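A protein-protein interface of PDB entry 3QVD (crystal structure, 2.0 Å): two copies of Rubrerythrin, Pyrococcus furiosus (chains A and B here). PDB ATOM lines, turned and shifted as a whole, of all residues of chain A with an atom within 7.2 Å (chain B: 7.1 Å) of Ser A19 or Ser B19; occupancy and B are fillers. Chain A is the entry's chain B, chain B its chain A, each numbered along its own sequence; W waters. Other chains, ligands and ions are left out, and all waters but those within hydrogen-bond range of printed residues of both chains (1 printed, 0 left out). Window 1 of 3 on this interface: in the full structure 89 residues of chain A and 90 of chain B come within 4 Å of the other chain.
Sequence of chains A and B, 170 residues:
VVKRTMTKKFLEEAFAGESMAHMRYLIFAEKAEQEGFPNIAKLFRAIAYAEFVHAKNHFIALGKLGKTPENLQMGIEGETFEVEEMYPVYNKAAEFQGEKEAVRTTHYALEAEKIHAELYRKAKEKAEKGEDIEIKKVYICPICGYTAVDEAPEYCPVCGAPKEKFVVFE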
ATOM      1  N   GLU A  13      -2.301   7.713  34.556  1.00  0.00           N
ATOM      2  CA  GLU A  13      -1.473   8.673  35.286  1.00  0.00           C
ATOM      3  C   GLU A  13      -0.251   9.075  34.458  1.00  0.00           C
ATOM      4  O   GLU A  13       0.135  10.252  34.429  1.00  0.00           O
ATOM      5  CB  GLU A  13      -1.029   8.077  36.624  1.00  0.00           C
ATOM      6  CG  GLU A  13      -2.163   7.957  37.628  1.00  0.00           C
ATOM      7  CD  GLU A  13      -1.736   7.312  38.937  1.00  0.00           C
ATOM      8  OE1 GLU A  13      -0.757   7.789  39.548  1.00  0.00           O
ATOM      9  OE2 GLU A  13      -2.387   6.335  39.357  1.00  0.00           O
ATOM     10  N   ALA A  14       0.360   8.102  33.782  1.00  0.00           N
ATOM     11  CA  ALA A  14       1.528   8.381  32.951  1.00  0.00           C
ATOM     12  C   ALA A  14       1.123   9.258  31.762  1.00  0.00           C
ATOM     13  O   ALA A  14       1.870  10.152  31.356  1.00  0.00           O
ATOM     14  CB  ALA A  14       2.153   7.076  32.464  1.00  0.00           C
ATOM     15  N   PHE A  15      -0.060   9.004  31.204  1.00  0.00           N
ATOM     16  CA  PHE A  15      -0.546   9.802  30.080  1.00  0.00           C
ATOM     17  C   PHE A  15      -0.690  11.262  30.515  1.00  0.00           C
ATOM     18  O   PHE A  15      -0.367  12.185  29.764  1.00  0.00           O
ATOM     19  CB  PHE A  15      -1.910   9.299  29.585  1.00  0.00           C
ATOM     20  CG  PHE A  15      -2.473  10.115  28.444  1.00  0.00           C
ATOM     21  CD1 PHE A  15      -1.907  10.041  27.174  1.00  0.00           C
ATOM     22  CD2 PHE A  15      -3.511  11.011  28.657  1.00  0.00           C
ATOM     23  CE1 PHE A  15      -2.365  10.854  26.134  1.00  0.00           C
ATOM     24  CE2 PHE A  15      -3.981  11.830  27.626  1.00  0.00           C
ATOM     25  CZ  PHE A  15      -3.404  11.751  26.364  1.00  0.00           C
ATOM     26  N   ALA A  16      -1.202  11.470  31.721  1.00  0.00           N
ATOM     27  CA  ALA A  16      -1.363  12.824  32.232  1.00  0.00           C
ATOM     28  C   ALA A  16       0.022  13.432  32.464  1.00  0.00           C
ATOM     29  O   ALA A  16       0.254  14.600  32.163  1.00  0.00           O
ATOM     30  CB  ALA A  16      -2.158  12.803  33.528  1.00  0.00           C
ATOM     31  N   GLY A  17       0.937  12.621  32.991  1.00  0.00           N
ATOM     32  CA  GLY A  17       2.293  13.078  33.265  1.00  0.00           C
ATOM     33  C   GLY A  17       3.050  13.495  32.020  1.00  0.00           C
ATOM     34  O   GLY A  17       3.721  14.532  32.012  1.00  0.00           O
ATOM     35  N   GLU A  18       2.951  12.676  30.975  1.00  0.00           N
ATOM     36  CA  GLU A  18       3.599  12.948  29.692  1.00  0.00           C
ATOM     37  C   GLU A  18       2.971  14.174  29.032  1.00  0.00           C
ATOM     38  O   GLU A  18       3.663  14.985  28.422  1.00  0.00           O
ATOM     39  CB  GLU A  18       3.436  11.748  28.748  1.00  0.00           C
ATOM     40  CG  GLU A  18       4.203  10.493  29.144  1.00  0.00           C
ATOM     41  CD  GLU A  18       5.701  10.668  29.023  1.00  0.00           C
ATOM     42  OE1 GLU A  18       6.135  11.587  28.294  1.00  0.00           O
ATOM     43  OE2 GLU A  18       6.444   9.877  29.639  1.00  0.00           O
ATOM     44  N   SER A  19       1.647  14.293  29.137  1.00  0.00           N
ATOM     45  CA  SER A  19       0.938  15.430  28.547  1.00  0.00           C
ATOM     46  C   SER A  19       1.381  16.747  29.195  1.00  0.00           C
ATOM     47  O   SER A  19       1.615  17.734  28.505  1.00  0.00           O
ATOM     48  CB  SER A  19      -0.579  15.255  28.708  1.00  0.00           C
ATOM     49  OG  SER A  19      -1.051  14.172  27.915  1.00  0.00           O
ATOM     50  N   MET A  20       1.487  16.762  30.522  1.00  0.00           N
ATOM     51  CA  MET A  20       1.912  17.975  31.226  1.00  0.00           C
ATOM     52  C   MET A  20       3.384  18.296  30.974  1.00  0.00           C
ATOM     53  O   MET A  20       3.764  19.466  30.913  1.00  0.00           O
ATOM     54  CB  MET A  20       1.645  17.847  32.730  1.00  0.00           C
ATOM     55  CG  MET A  20       0.168  17.994  33.083  1.00  0.00           C
ATOM     56  SD  MET A  20      -0.179  18.016  34.854  1.00  0.00           S
ATOM     57  CE  MET A  20       0.092  16.306  35.244  1.00  0.00           C
ATOM     58  N   ALA A  21       4.213  17.264  30.821  1.00  0.00           N
ATOM     59  CA  ALA A  21       5.632  17.477  30.541  1.00  0.00           C
ATOM     60  C   ALA A  21       5.742  18.079  29.134  1.00  0.00           C
ATOM     61  O   ALA A  21       6.467  19.046  28.914  1.00  0.00           O
ATOM     62  CB  ALA A  21       6.388  16.156  30.617  1.00  0.00           C
ATOM     63  N   HIS A  22       5.006  17.499  28.191  1.00  0.00           N
ATOM     64  CA  HIS A  22       4.978  17.983  26.815  1.00  0.00           C
ATOM     65  C   HIS A  22       4.605  19.464  26.808  1.00  0.00           C
ATOM     66  O   HIS A  22       5.246  20.272  26.147  1.00  0.00           O
ATOM     67  CB  HIS A  22       3.929  17.201  26.009  1.00  0.00           C
ATOM     68  CG  HIS A  22       3.652  17.779  24.654  1.00  0.00           C
ATOM     69  ND1 HIS A  22       4.425  17.493  23.549  1.00  0.00           N
ATOM     70  CD2 HIS A  22       2.703  18.649  24.235  1.00  0.00           C
ATOM     71  CE1 HIS A  22       3.964  18.163  22.507  1.00  0.00           C
ATOM     72  NE2 HIS A  22       2.919  18.873  22.897  1.00  0.00           N
ATOM     73  N   MET A  23       3.566  19.808  27.562  1.00  0.00           N
ATOM     74  CA  MET A  23       3.076  21.180  27.639  1.00  0.00           C
ATOM     75  C   MET A  23       4.092  22.132  28.276  1.00  0.00           C
ATOM     76  O   MET A  23       4.371  23.205  27.738  1.00  0.00           O
ATOM     77  CB  MET A  23       1.758  21.216  28.423  1.00  0.00           C
ATOM     78  CG  MET A  23       1.042  22.564  28.427  1.00  0.00           C
ATOM     79  SD  MET A  23       0.673  23.190  26.767  1.00  0.00           S
ATOM     80  CE  MET A  23      -0.788  22.168  26.313  1.00  0.00           C
ATOM     81  N   ARG A  24       4.639  21.745  29.420  1.00  0.00           N
ATOM     82  CA  ARG A  24       5.627  22.595  30.079  1.00  0.00           C
ATOM     83  C   ARG A  24       6.797  22.883  29.137  1.00  0.00           C
ATOM     84  O   ARG A  24       7.298  24.008  29.079  1.00  0.00           O
ATOM     85  CB  ARG A  24       6.137  21.926  31.359  1.00  0.00           C
ATOM     86  CG  ARG A  24       5.130  21.920  32.503  1.00  0.00           C
ATOM     87  CD  ARG A  24       5.810  21.565  33.830  1.00  0.00           C
ATOM     88  NE  ARG A  24       6.344  20.210  33.813  1.00  0.00           N
ATOM     89  CZ  ARG A  24       5.667  19.128  34.189  1.00  0.00           C
ATOM     90  NH1 ARG A  24       6.239  17.938  34.126  1.00  0.00           N
ATOM     91  NH2 ARG A  24       4.429  19.240  34.654  1.00  0.00           N
ATOM     92  N   TYR A  25       7.224  21.869  28.393  1.00  0.00           N
ATOM     93  CA  TYR A  25       8.341  22.031  27.470  1.00  0.00           C
ATOM     94  C   TYR A  25       8.005  22.967  26.306  1.00  0.00           C
ATOM     95  O   TYR A  25       8.864  23.729  25.864  1.00  0.00           O
ATOM     96  CB  TYR A  25       8.814  20.655  26.966  1.00  0.00           C
ATOM     97  CG  TYR A  25       9.372  19.774  28.080  1.00  0.00           C
ATOM     98  CD1 TYR A  25       9.528  18.399  27.901  1.00  0.00           C
ATOM     99  CD2 TYR A  25       9.720  20.321  29.322  1.00  0.00           C
ATOM    100  CE1 TYR A  25      10.012  17.584  28.939  1.00  0.00           C
ATOM    101  CE2 TYR A  25      10.205  19.518  30.359  1.00  0.00           C
ATOM    102  CZ  TYR A  25      10.346  18.154  30.162  1.00  0.00           C
ATOM    103  OH  TYR A  25      10.814  17.364  31.190  1.00  0.00           O
ATOM    104  N   ILE A  27       5.971  25.398  26.529  1.00  0.00           N
ATOM    105  CA  ILE A  27       5.932  26.693  27.190  1.00  0.00           C
ATOM    106  C   ILE A  27       7.362  27.180  27.447  1.00  0.00           C
ATOM    107  O   ILE A  27       7.685  28.337  27.188  1.00  0.00           O
ATOM    108  CB  ILE A  27       5.161  26.603  28.534  1.00  0.00           C
ATOM    109  CG1 ILE A  27       3.680  26.313  28.270  1.00  0.00           C
ATOM    110  CG2 ILE A  27       5.292  27.909  29.314  1.00  0.00           C
ATOM    111  CD1 ILE A  27       2.877  25.989  29.536  1.00  0.00           C
ATOM    112  N   GLU A  51       7.871  13.355  24.303  1.00  0.00           N
ATOM    113  CA  GLU A  51       6.843  13.094  25.312  1.00  0.00           C
ATOM    114  C   GLU A  51       5.492  12.835  24.621  1.00  0.00           C
ATOM    115  O   GLU A  51       4.622  12.165  25.180  1.00  0.00           O
ATOM    116  CB  GLU A  51       6.743  14.271  26.292  1.00  0.00           C
ATOM    117  CG  GLU A  51       8.099  14.847  26.728  1.00  0.00           C
ATOM    118  CD  GLU A  51       8.976  13.883  27.527  1.00  0.00           C
ATOM    119  OE1 GLU A  51       8.849  12.656  27.359  1.00  0.00           O
ATOM    120  OE2 GLU A  51       9.825  14.361  28.317  1.00  0.00           O
ATOM    121  N   PHE A  52       5.323  13.368  23.409  1.00  0.00           N
ATOM    122  CA  PHE A  52       4.097  13.144  22.632  1.00  0.00           C
ATOM    123  C   PHE A  52       4.094  11.666  22.228  1.00  0.00           C
ATOM    124  O   PHE A  52       3.067  10.990  22.295  1.00  0.00           O
ATOM    125  CB  PHE A  52       4.079  14.034  21.379  1.00  0.00           C
ATOM    126  CG  PHE A  52       3.242  13.484  20.240  1.00  0.00           C
ATOM    127  CD1 PHE A  52       1.864  13.686  20.202  1.00  0.00           C
ATOM    128  CD2 PHE A  52       3.839  12.747  19.218  1.00  0.00           C
ATOM    129  CE1 PHE A  52       1.087  13.155  19.161  1.00  0.00           C
ATOM    130  CE2 PHE A  52       3.074  12.210  18.171  1.00  0.00           C
ATOM    131  CZ  PHE A  52       1.694  12.416  18.146  1.00  0.00           C
ATOM    132  N   ALA A  55       3.221   9.637  25.331  1.00  0.00           N
ATOM    133  CA  ALA A  55       1.803   9.735  25.665  1.00  0.00           C
ATOM    134  C   ALA A  55       0.968   8.970  24.641  1.00  0.00           C
ATOM    135  O   ALA A  55       0.045   8.241  24.998  1.00  0.00           O
ATOM    136  CB  ALA A  55       1.369  11.194  25.711  1.00  0.00           C
ATOM    137  N   LYS A  56       1.290   9.143  23.363  1.00  0.00           N
ATOM    138  CA  LYS A  56       0.555   8.445  22.321  1.00  0.00           C
ATOM    139  C   LYS A  56       0.645   6.944  22.562  1.00  0.00           C
ATOM    140  O   LYS A  56      -0.340   6.229  22.397  1.00  0.00           O
ATOM    141  CB  LYS A  56       1.102   8.781  20.928  1.00  0.00           C
ATOM    142  CG  LYS A  56       0.343   8.050  19.820  1.00  0.00           C
ATOM    143  CD  LYS A  56       0.654   8.578  18.427  1.00  0.00           C
ATOM    144  CE  LYS A  56       2.038   8.182  17.961  1.00  0.00           C
ATOM    145  NZ  LYS A  56       2.233   8.528  16.520  1.00  0.00           N
ATOM    146  N   GLU B  13      -5.597  21.450  38.184  1.00  0.00           N
ATOM    147  CA  GLU B  13      -6.394  20.428  37.501  1.00  0.00           C
ATOM    148  C   GLU B  13      -6.702  20.869  36.063  1.00  0.00           C
ATOM    149  O   GLU B  13      -6.676  20.056  35.135  1.00  0.00           O
ATOM    150  CB  GLU B  13      -7.697  20.174  38.268  1.00  0.00           C
ATOM    151  CG  GLU B  13      -7.456  19.752  39.713  1.00  0.00           C
ATOM    152  CD  GLU B  13      -8.731  19.605  40.524  1.00  0.00           C
ATOM    153  OE1 GLU B  13      -9.586  20.518  40.475  1.00  0.00           O
ATOM    154  OE2 GLU B  13      -8.869  18.579  41.224  1.00  0.00           O
ATOM    155  N   ALA B  14      -6.992  22.158  35.885  1.00  0.00           N
ATOM    156  CA  ALA B  14      -7.291  22.705  34.562  1.00  0.00           C
ATOM    157  C   ALA B  14      -6.057  22.630  33.658  1.00  0.00           C
ATOM    158  O   ALA B  14      -6.180  22.418  32.446  1.00  0.00           O
ATOM    159  CB  ALA B  14      -7.773  24.165  34.683  1.00  0.00           C
ATOM    160  N   PHE B  15      -4.875  22.822  34.240  1.00  0.00           N
ATOM    161  CA  PHE B  15      -3.635  22.744  33.470  1.00  0.00           C
ATOM    162  C   PHE B  15      -3.472  21.309  32.963  1.00  0.00           C
ATOM    163  O   PHE B  15      -3.113  21.083  31.809  1.00  0.00           O
ATOM    164  CB  PHE B  15      -2.425  23.126  34.335  1.00  0.00           C
ATOM    165  CG  PHE B  15      -1.100  22.906  33.650  1.00  0.00           C
ATOM    166  CD1 PHE B  15      -0.653  23.782  32.663  1.00  0.00           C
ATOM    167  CD2 PHE B  15      -0.319  21.792  33.958  1.00  0.00           C
ATOM    168  CE1 PHE B  15       0.549  23.552  31.986  1.00  0.00           C
ATOM    169  CE2 PHE B  15       0.884  21.553  33.289  1.00  0.00           C
ATOM    170  CZ  PHE B  15       1.319  22.440  32.297  1.00  0.00           C
ATOM    171  N   ALA B  16      -3.736  20.343  33.841  1.00  0.00           N
ATOM    172  CA  ALA B  16      -3.644  18.937  33.487  1.00  0.00           C
ATOM    173  C   ALA B  16      -4.705  18.612  32.425  1.00  0.00           C
ATOM    174  O   ALA B  16      -4.427  17.904  31.462  1.00  0.00           O
ATOM    175  CB  ALA B  16      -3.856  18.068  34.729  1.00  0.00           C
ATOM    176  N   GLY B  17      -5.913  19.143  32.602  1.00  0.00           N
ATOM    177  CA  GLY B  17      -6.989  18.895  31.648  1.00  0.00           C
ATOM    178  C   GLY B  17      -6.676  19.451  30.267  1.00  0.00           C
ATOM    179  O   GLY B  17      -6.901  18.795  29.246  1.00  0.00           O
ATOM    180  N   GLU B  18      -6.154  20.673  30.247  1.00  0.00           N
ATOM    181  CA  GLU B  18      -5.775  21.346  29.009  1.00  0.00           C
ATOM    182  C   GLU B  18      -4.625  20.608  28.329  1.00  0.00           C
ATOM    183  O   GLU B  18      -4.598  20.484  27.103  1.00  0.00           O
ATOM    184  CB  GLU B  18      -5.346  22.784  29.309  1.00  0.00           C
ATOM    185  CG  GLU B  18      -6.490  23.700  29.727  1.00  0.00           C
ATOM    186  CD  GLU B  18      -7.430  24.010  28.578  1.00  0.00           C
ATOM    187  OE1 GLU B  18      -8.555  24.469  28.846  1.00  0.00           O
ATOM    188  OE2 GLU B  18      -7.038  23.801  27.406  1.00  0.00           O
ATOM    189  N   SER B  19      -3.670  20.127  29.128  1.00  0.00           N
ATOM    190  CA  SER B  19      -2.524  19.407  28.587  1.00  0.00           C
ATOM    191  C   SER B  19      -2.960  18.115  27.906  1.00  0.00           C
ATOM    192  O   SER B  19      -2.467  17.777  26.829  1.00  0.00           O
ATOM    193  CB  SER B  19      -1.508  19.086  29.695  1.00  0.00           C
ATOM    194  OG  SER B  19      -0.935  20.270  30.228  1.00  0.00           O
ATOM    195  N   MET B  20      -3.886  17.392  28.531  1.00  0.00           N
ATOM    196  CA  MET B  20      -4.361  16.143  27.951  1.00  0.00           C
ATOM    197  C   MET B  20      -5.241  16.365  26.722  1.00  0.00           C
ATOM    198  O   MET B  20      -5.197  15.575  25.780  1.00  0.00           O
ATOM    199  CB  MET B  20      -5.099  15.316  29.001  1.00  0.00           C
ATOM    200  CG  MET B  20      -4.152  14.734  30.053  1.00  0.00           C
ATOM    201  SD  MET B  20      -4.963  13.639  31.224  1.00  0.00           S
ATOM    202  CE  MET B  20      -5.731  14.830  32.325  1.00  0.00           C
ATOM    203  N   ALA B  21      -6.028  17.434  26.732  1.00  0.00           N
ATOM    204  CA  ALA B  21      -6.889  17.752  25.592  1.00  0.00           C
ATOM    205  C   ALA B  21      -5.988  18.095  24.399  1.00  0.00           C
ATOM    206  O   ALA B  21      -6.224  17.647  23.280  1.00  0.00           O
ATOM    207  CB  ALA B  21      -7.796  18.934  25.928  1.00  0.00           C
ATOM    208  N   HIS B  22      -4.956  18.889  24.655  1.00  0.00           N
ATOM    209  CA  HIS B  22      -3.997  19.278  23.626  1.00  0.00           C
ATOM    210  C   HIS B  22      -3.318  18.028  23.055  1.00  0.00           C
ATOM    211  O   HIS B  22      -3.185  17.874  21.834  1.00  0.00           O
ATOM    212  CB  HIS B  22      -2.957  20.231  24.240  1.00  0.00           C
ATOM    213  CG  HIS B  22      -1.753  20.465  23.381  1.00  0.00           C
ATOM    214  ND1 HIS B  22      -0.651  19.637  23.398  1.00  0.00           N
ATOM    215  CD2 HIS B  22      -1.479  21.433  22.476  1.00  0.00           C
ATOM    216  CE1 HIS B  22       0.249  20.086  22.543  1.00  0.00           C
ATOM    217  NE2 HIS B  22      -0.229  21.174  21.969  1.00  0.00           N
ATOM    218  N   MET B  23      -2.916  17.124  23.943  1.00  0.00           N
ATOM    219  CA  MET B  23      -2.249  15.895  23.537  1.00  0.00           C
ATOM    220  C   MET B  23      -3.168  15.011  22.697  1.00  0.00           C
ATOM    221  O   MET B  23      -2.768  14.508  21.649  1.00  0.00           O
ATOM    222  CB  MET B  23      -1.763  15.123  24.773  1.00  0.00           C
ATOM    223  CG  MET B  23      -0.946  13.872  24.448  1.00  0.00           C
ATOM    224  SD  MET B  23       0.550  14.218  23.476  1.00  0.00           S
ATOM    225  CE  MET B  23       1.666  14.858  24.756  1.00  0.00           C
ATOM    226  N   ARG B  24      -4.394  14.810  23.156  1.00  0.00           N
ATOM    227  CA  ARG B  24      -5.330  13.989  22.401  1.00  0.00           C
ATOM    228  C   ARG B  24      -5.532  14.558  20.987  1.00  0.00           C
ATOM    229  O   ARG B  24      -5.562  13.820  20.006  1.00  0.00           O
ATOM    230  CB  ARG B  24      -6.674  13.901  23.133  1.00  0.00           C
ATOM    231  CG  ARG B  24      -6.650  13.026  24.387  1.00  0.00           C
ATOM    232  CD  ARG B  24      -8.066  12.702  24.870  1.00  0.00           C
ATOM    233  NE  ARG B  24      -8.785  13.901  25.291  1.00  0.00           N
ATOM    234  CZ  ARG B  24      -8.748  14.411  26.518  1.00  0.00           C
ATOM    235  NH1 ARG B  24      -9.431  15.516  26.796  1.00  0.00           N
ATOM    236  NH2 ARG B  24      -8.051  13.808  27.473  1.00  0.00           N
ATOM    237  N   TYR B  25      -5.656  15.874  20.885  1.00  0.00           N
ATOM    238  CA  TYR B  25      -5.867  16.500  19.589  1.00  0.00           C
ATOM    239  C   TYR B  25      -4.693  16.318  18.626  1.00  0.00           C
ATOM    240  O   TYR B  25      -4.899  16.205  17.416  1.00  0.00           O
ATOM    241  CB  TYR B  25      -6.212  17.979  19.780  1.00  0.00           C
ATOM    242  CG  TYR B  25      -7.502  18.198  20.555  1.00  0.00           C
ATOM    243  CD1 TYR B  25      -7.786  19.433  21.137  1.00  0.00           C
ATOM    244  CD2 TYR B  25      -8.434  17.165  20.715  1.00  0.00           C
ATOM    245  CE1 TYR B  25      -8.964  19.637  21.863  1.00  0.00           C
ATOM    246  CE2 TYR B  25      -9.615  17.360  21.435  1.00  0.00           C
ATOM    247  CZ  TYR B  25      -9.871  18.598  22.007  1.00  0.00           C
ATOM    248  OH  TYR B  25     -11.029  18.800  22.725  1.00  0.00           O
ATOM    249  N   ILE B  27      -2.760  13.714  18.653  1.00  0.00           N
ATOM    250  CA  ILE B  27      -2.865  12.301  18.304  1.00  0.00           C
ATOM    251  C   ILE B  27      -3.968  12.115  17.253  1.00  0.00           C
ATOM    252  O   ILE B  27      -3.784  11.412  16.256  1.00  0.00           O
ATOM    253  CB  ILE B  27      -3.196  11.455  19.563  1.00  0.00           C
ATOM    254  CG1 ILE B  27      -2.056  11.579  20.581  1.00  0.00           C
ATOM    255  CG2 ILE B  27      -3.422   9.997  19.184  1.00  0.00           C
ATOM    256  CD1 ILE B  27      -2.291  10.819  21.892  1.00  0.00           C
ATOM    257  N   GLU B  51      -5.433  25.073  23.029  1.00  0.00           N
ATOM    258  CA  GLU B  51      -5.364  24.475  24.366  1.00  0.00           C
ATOM    259  C   GLU B  51      -4.007  24.794  25.001  1.00  0.00           C
ATOM    260  O   GLU B  51      -3.887  24.890  26.226  1.00  0.00           O
ATOM    261  CB  GLU B  51      -5.563  22.956  24.301  1.00  0.00           C
ATOM    262  CG  GLU B  51      -6.751  22.465  23.450  1.00  0.00           C
ATOM    263  CD  GLU B  51      -8.109  23.070  23.822  1.00  0.00           C
ATOM    264  OE1 GLU B  51      -9.142  22.537  23.359  1.00  0.00           O
ATOM    265  OE2 GLU B  51      -8.164  24.075  24.556  1.00  0.00           O
ATOM    266  N   PHE B  52      -2.984  24.935  24.160  1.00  0.00           N
ATOM    267  CA  PHE B  52      -1.645  25.290  24.622  1.00  0.00           C
ATOM    268  C   PHE B  52      -1.740  26.673  25.274  1.00  0.00           C
ATOM    269  O   PHE B  52      -1.155  26.923  26.324  1.00  0.00           O
ATOM    270  CB  PHE B  52      -0.675  25.342  23.431  1.00  0.00           C
ATOM    271  CG  PHE B  52       0.536  26.212  23.667  1.00  0.00           C
ATOM    272  CD1 PHE B  52       1.610  25.753  24.424  1.00  0.00           C
ATOM    273  CD2 PHE B  52       0.585  27.504  23.153  1.00  0.00           C
ATOM    274  CE1 PHE B  52       2.715  26.568  24.667  1.00  0.00           C
ATOM    275  CE2 PHE B  52       1.684  28.332  23.393  1.00  0.00           C
ATOM    276  CZ  PHE B  52       2.751  27.863  24.151  1.00  0.00           C
ATOM    277  N   ALA B  55      -3.555  26.314  28.651  1.00  0.00           N
ATOM    278  CA  ALA B  55      -2.638  25.696  29.608  1.00  0.00           C
ATOM    279  C   ALA B  55      -1.572  26.691  30.063  1.00  0.00           C
ATOM    280  O   ALA B  55      -1.333  26.849  31.260  1.00  0.00           O
ATOM    281  CB  ALA B  55      -1.973  24.477  28.981  1.00  0.00           C
HETATM  282  O   HOH W   1       0.118  18.174  26.209  1.00  0.00           O
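Hydrophobic or aromatic side chains of chain B within 4 Å of the printed part of chain A: Phe B15, Ala B16, Met B20, His B22, Met B23, Ile B27, Phe B52 and Ala B55.
Of the 18 printed residues of chain A, 11 touch a printed residue of chain B.
Hydrophobic or aromatic side chains of chain A within 4 Å of the printed part of chain B: Phe A15, Ala A16, Met A20, His A22, Met A23, Ile A27, Phe A52 and Ala A55.
Among the printed residues, pairs that only touch across the chains: His A22 with His B22, Ser A19 with Met B23, Met A23 with Ser B19, His A22 with Met B23, Met A23 with His B22, Phe A52 with Met B23, Met A23 with Phe B52, Ser A19 with Ser B19, Met A23 with Ala B55, Met A20 with Phe B15, Met A20 with Ala B16, Ala A16 with Met B20, Met A23 with Phe B15, Lys A56 with Ile B27, Phe A15 with Met B23, Ile A27 with Phe B52, Ala A55 with Met B23, Phe A15 with Met B20, Met A20 with Ser B19, Phe A52 with Ile B27, Ser A19 with Met B20 and Arg A24 with Phe B15.
Of the printed residues of chain B, Phe A15 touches Met B20 (3.8 Å) and Met B23 (3.7 Å).
Ser A19 touches just these residues of chain B: Ser B19, Met B20 and Met B23.
Of the printed residues of chain B, His A22 touches His B22 and Met B23.
Tyr A25 touches none of the printed residues of chain B.
Ser B19 touches three residues of chain A.
The nearest residue of chain A that does not touch Ser B19 is Ala A16 (5.4 Å).
Phe A15 touches Met B23, and with the chains exchanged Met A23 touches Phe B15.
Met A23 touches Phe B52, and with the chains exchanged Phe A52 touches Met B23.
Met A23 touches Ala B55, and with the chains exchanged Ala A55 touches Met B23.
Arg A24 touches Phe B15, but with the chains exchanged Phe A15 does not touch Arg B24 (4.01 Å).
17 positions are printed for both chains.
The backbone carbonyl oxygen of Phe B15 lies within hydrogen-bond range of the side-chain hydroxyl of Ser B19 (2.8 Å).
O of Phe A15 sits at hydrogen-bond distance from OG of Ser A19, 2.8 Å away.
Water W1 lies within hydrogen-bond range of O of Ser B19 (2.7 Å), O of Ser A19 (2.8 Å) and ND1 of His B22 (3.3 Å).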
